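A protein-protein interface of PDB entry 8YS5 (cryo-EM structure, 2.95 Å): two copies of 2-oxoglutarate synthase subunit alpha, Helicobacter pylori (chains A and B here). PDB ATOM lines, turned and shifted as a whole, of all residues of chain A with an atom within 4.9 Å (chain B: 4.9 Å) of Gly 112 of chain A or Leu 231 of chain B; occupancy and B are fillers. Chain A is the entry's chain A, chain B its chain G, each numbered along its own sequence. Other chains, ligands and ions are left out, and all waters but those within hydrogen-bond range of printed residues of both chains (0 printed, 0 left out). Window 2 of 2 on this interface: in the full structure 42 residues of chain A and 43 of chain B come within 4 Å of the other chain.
The backbone NH (N) of Gly 112 of chain A is in hydrogen-bond range of the backbone carbonyl oxygen (O) of Gly 230 of chain B (3.4 Å). O of Gly 230 of chain B lies close to O of Ser 110 of chain A (3.1 Å).
A ring nitrogen (ND1) of His 233 of chain B is in hydrogen-bond range of the backbone carbonyl oxygen (O) of Leu 231 of chain B (2.9 Å).
Among the printed residues, pairs that only touch across the chains: Thr 111 of chain A with Gly 230 of chain B (3.7 Å), Thr 111 of chain A with Leu 231 of chain B (3.2 Å), Gly 112 of chain A with Leu 231 of chain B (3.3 Å), Gly 112 of chain A with His 232 of chain B (3.3 Å) and Met 113 of chain A with His 232 of chain B (3.5 Å).
Printed residues of chain B within 4 Å of Ser 110 of chain A: Gly 230. Of the printed residues of chain B, Thr 111 of chain A touches Gly 230 (3.7 Å) and Leu 231 (3.2 Å). Gly 112 of chain A touches just these residues of chain B: Gly 230, Leu 231 and His 232. Of the printed residues of chain B, Met 113 of chain A touches His 232 (3.5 Å). Ser 229 of chain B touches none of the printed residues of chain A. Of the printed residues of chain A, Gly 230 of chain B touches Ser 110, Thr 111 and Gly 112. Leu 231 of chain B touches just these residues of chain A: Thr 111 (3.2 Å) and Gly 112 (3.3 Å). Printed residues of chain A within 4 Å of His 232 of chain B: Gly 112 (3.3 Å) and Met 113 (3.5 Å). The nearest printed residue of chain B that does not touch Gly 112 of chain A is Met 94 of chain B (4.9 Å).
Printed residues of chain B that touch a printed residue of chain A: Gly 230, Leu 231 and His 232. Hydrophobic or aromatic side chains of chain B that line the printed part of chain A: Leu 231 and His 232. Among the printed residues, 7 pairs touch across the chains.
No position is printed for both chains. Of the 7 pairs that touch across the chains among the printed residues, none has its exchanged pair printed and touching as well.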
ATOM      1  N   SER A 107      14.420 -17.536 -11.926  1.00  0.00           N
ATOM      2  CA  SER A 107      13.361 -16.665 -11.425  1.00  0.00           C
ATOM      3  C   SER A 107      13.924 -15.727 -10.364  1.00  0.00           C
ATOM      4  O   SER A 107      14.103 -16.114  -9.206  1.00  0.00           O
ATOM      5  CB  SER A 107      12.208 -17.493 -10.872  1.00  0.00           C
ATOM      6  OG  SER A 107      10.991 -16.770 -10.931  1.00  0.00           O
ATOM      7  N   SER A 110      15.868 -12.352  -5.458  1.00  0.00           N
ATOM      8  CA  SER A 110      16.646 -13.267  -4.628  1.00  0.00           C
ATOM      9  C   SER A 110      15.841 -14.520  -4.307  1.00  0.00           C
ATOM     10  O   SER A 110      14.614 -14.525  -4.454  1.00  0.00           O
ATOM     11  CB  SER A 110      17.094 -12.575  -3.339  1.00  0.00           C
ATOM     12  OG  SER A 110      16.133 -12.740  -2.311  1.00  0.00           O
ATOM     13  N   THR A 111      16.500 -15.549  -3.772  1.00  0.00           N
ATOM     14  CA  THR A 111      16.364 -16.928  -4.233  1.00  0.00           C
ATOM     15  C   THR A 111      15.020 -17.239  -4.884  1.00  0.00           C
ATOM     16  O   THR A 111      14.993 -17.762  -6.002  1.00  0.00           O
ATOM     17  CB  THR A 111      16.585 -17.881  -3.056  1.00  0.00           C
ATOM     18  OG1 THR A 111      15.627 -17.604  -2.028  1.00  0.00           O
ATOM     19  CG2 THR A 111      17.986 -17.724  -2.493  1.00  0.00           C
ATOM     20  N   GLY A 112      13.910 -16.921  -4.226  1.00  0.00           N
ATOM     21  CA  GLY A 112      12.622 -17.025  -4.886  1.00  0.00           C
ATOM     22  C   GLY A 112      12.263 -18.421  -5.357  1.00  0.00           C
ATOM     23  O   GLY A 112      11.949 -19.298  -4.547  1.00  0.00           O
ATOM     24  N   MET A 113      12.304 -18.635  -6.672  1.00  0.00           N
ATOM     25  CA  MET A 113      11.952 -19.913  -7.293  1.00  0.00           C
ATOM     26  C   MET A 113      13.175 -20.432  -8.036  1.00  0.00           C
ATOM     27  O   MET A 113      13.352 -20.153  -9.232  1.00  0.00           O
ATOM     28  CB  MET A 113      10.763 -19.752  -8.238  1.00  0.00           C
ATOM     29  CG  MET A 113       9.459 -19.386  -7.550  1.00  0.00           C
ATOM     30  SD  MET A 113       8.225 -18.781  -8.716  1.00  0.00           S
ATOM     31  CE  MET A 113       6.740 -18.883  -7.725  1.00  0.00           C
ATOM     32  N   PRO A 114      14.046 -21.195  -7.368  1.00  0.00           N
ATOM     33  CA  PRO A 114      15.297 -21.632  -8.010  1.00  0.00           C
ATOM     34  C   PRO A 114      15.105 -22.589  -9.176  1.00  0.00           C
ATOM     35  O   PRO A 114      16.032 -22.736  -9.984  1.00  0.00           O
ATOM     36  CB  PRO A 114      16.059 -22.311  -6.865  1.00  0.00           C
ATOM     37  CG  PRO A 114      15.009 -22.701  -5.882  1.00  0.00           C
ATOM     38  CD  PRO A 114      13.949 -21.649  -5.971  1.00  0.00           C
ATOM     39  N   MET B  94      12.745  -8.168  -1.118  1.00  0.00           N
ATOM     40  CA  MET B  94      11.803  -9.276  -1.205  1.00  0.00           C
ATOM     41  C   MET B  94      11.132  -9.574   0.131  1.00  0.00           C
ATOM     42  O   MET B  94       9.928  -9.848   0.172  1.00  0.00           O
ATOM     43  CB  MET B  94      12.513 -10.526  -1.730  1.00  0.00           C
ATOM     44  CG  MET B  94      11.780 -11.824  -1.452  1.00  0.00           C
ATOM     45  SD  MET B  94      10.259 -11.978  -2.405  1.00  0.00           S
ATOM     46  CE  MET B  94      10.906 -12.495  -3.989  1.00  0.00           C
ATOM     47  N   SER B 229      11.842 -15.128   4.883  1.00  0.00           N
ATOM     48  CA  SER B 229      12.775 -15.738   3.945  1.00  0.00           C
ATOM     49  C   SER B 229      12.806 -14.896   2.677  1.00  0.00           C
ATOM     50  O   SER B 229      12.002 -13.978   2.497  1.00  0.00           O
ATOM     51  CB  SER B 229      12.389 -17.190   3.645  1.00  0.00           C
ATOM     52  OG  SER B 229      11.189 -17.254   2.897  1.00  0.00           O
ATOM     53  N   GLY B 230      13.749 -15.218   1.795  1.00  0.00           N
ATOM     54  CA  GLY B 230      13.868 -14.574   0.507  1.00  0.00           C
ATOM     55  C   GLY B 230      13.145 -15.266  -0.625  1.00  0.00           C
ATOM     56  O   GLY B 230      13.138 -14.749  -1.744  1.00  0.00           O
ATOM     57  N   LEU B 231      12.541 -16.422  -0.370  1.00  0.00           N
ATOM     58  CA  LEU B 231      11.786 -17.135  -1.387  1.00  0.00           C
ATOM     59  C   LEU B 231      10.403 -16.512  -1.556  1.00  0.00           C
ATOM     60  O   LEU B 231       9.954 -15.697  -0.744  1.00  0.00           O
ATOM     61  CB  LEU B 231      11.665 -18.613  -1.021  1.00  0.00           C
ATOM     62  CG  LEU B 231      12.836 -19.525  -1.394  1.00  0.00           C
ATOM     63  CD1 LEU B 231      13.844 -19.593  -0.263  1.00  0.00           C
ATOM     64  CD2 LEU B 231      12.335 -20.917  -1.743  1.00  0.00           C
ATOM     65  N   HIS B 232       9.721 -16.901  -2.630  1.00  0.00           N
ATOM     66  CA  HIS B 232       8.345 -16.465  -2.848  1.00  0.00           C
ATOM     67  C   HIS B 232       7.463 -17.071  -1.764  1.00  0.00           C
ATOM     68  O   HIS B 232       7.184 -18.274  -1.778  1.00  0.00           O
ATOM     69  CB  HIS B 232       7.863 -16.873  -4.237  1.00  0.00           C
ATOM     70  CG  HIS B 232       8.484 -16.090  -5.351  1.00  0.00           C
ATOM     71  ND1 HIS B 232       9.722 -15.493  -5.246  1.00  0.00           N
ATOM     72  CD2 HIS B 232       8.036 -15.803  -6.596  1.00  0.00           C
ATOM     73  CE1 HIS B 232      10.009 -14.875  -6.378  1.00  0.00           C
ATOM     74  NE2 HIS B 232       9.001 -15.048  -7.214  1.00  0.00           N
ATOM     75  N   HIS B 233       7.025 -16.241  -0.825  1.00  0.00           N
ATOM     76  CA  HIS B 233       6.327 -16.699   0.365  1.00  0.00           C
ATOM     77  C   HIS B 233       4.826 -16.458   0.254  1.00  0.00           C
ATOM     78  O   HIS B 233       4.351 -15.699  -0.593  1.00  0.00           O
ATOM     79  CB  HIS B 233       6.877 -15.997   1.608  1.00  0.00           C
ATOM     80  CG  HIS B 233       7.320 -14.591   1.360  1.00  0.00           C
ATOM     81  ND1 HIS B 233       8.648 -14.224   1.330  1.00  0.00           N
ATOM     82  CD2 HIS B 233       6.614 -13.461   1.126  1.00  0.00           C
ATOM     83  CE1 HIS B 233       8.741 -12.929   1.091  1.00  0.00           C
ATOM     84  NE2 HIS B 233       7.519 -12.441   0.963  1.00  0.00           N
ATOM     85  N   PRO B 239       7.764 -20.643   2.156  1.00  0.00           N
ATOM     86  CA  PRO B 239       8.020 -20.573   0.712  1.00  0.00           C
ATOM     87  C   PRO B 239       7.018 -21.391  -0.087  1.00  0.00           C
ATOM     88  O   PRO B 239       6.562 -22.454   0.341  1.00  0.00           O
ATOM     89  CB  PRO B 239       9.438 -21.138   0.575  1.00  0.00           C
ATOM     90  CG  PRO B 239       9.647 -21.951   1.807  1.00  0.00           C
ATOM     91  CD  PRO B 239       8.887 -21.251   2.887  1.00  0.00           C
ATOM     92  N   LEU B 249       2.790 -11.592  -5.704  1.00  0.00           N
ATOM     93  CA  LEU B 249       3.789 -11.012  -4.814  1.00  0.00           C
ATOM     94  C   LEU B 249       4.544  -9.879  -5.499  1.00  0.00           C
ATOM     95  O   LEU B 249       4.644  -8.770  -4.962  1.00  0.00           O
ATOM     96  CB  LEU B 249       4.755 -12.097  -4.338  1.00  0.00           C
ATOM     97  CG  LEU B 249       5.880 -11.646  -3.406  1.00  0.00           C
ATOM     98  CD1 LEU B 249       5.315 -10.929  -2.193  1.00  0.00           C
ATOM     99  CD2 LEU B 249       6.720 -12.835  -2.981  1.00  0.00           C
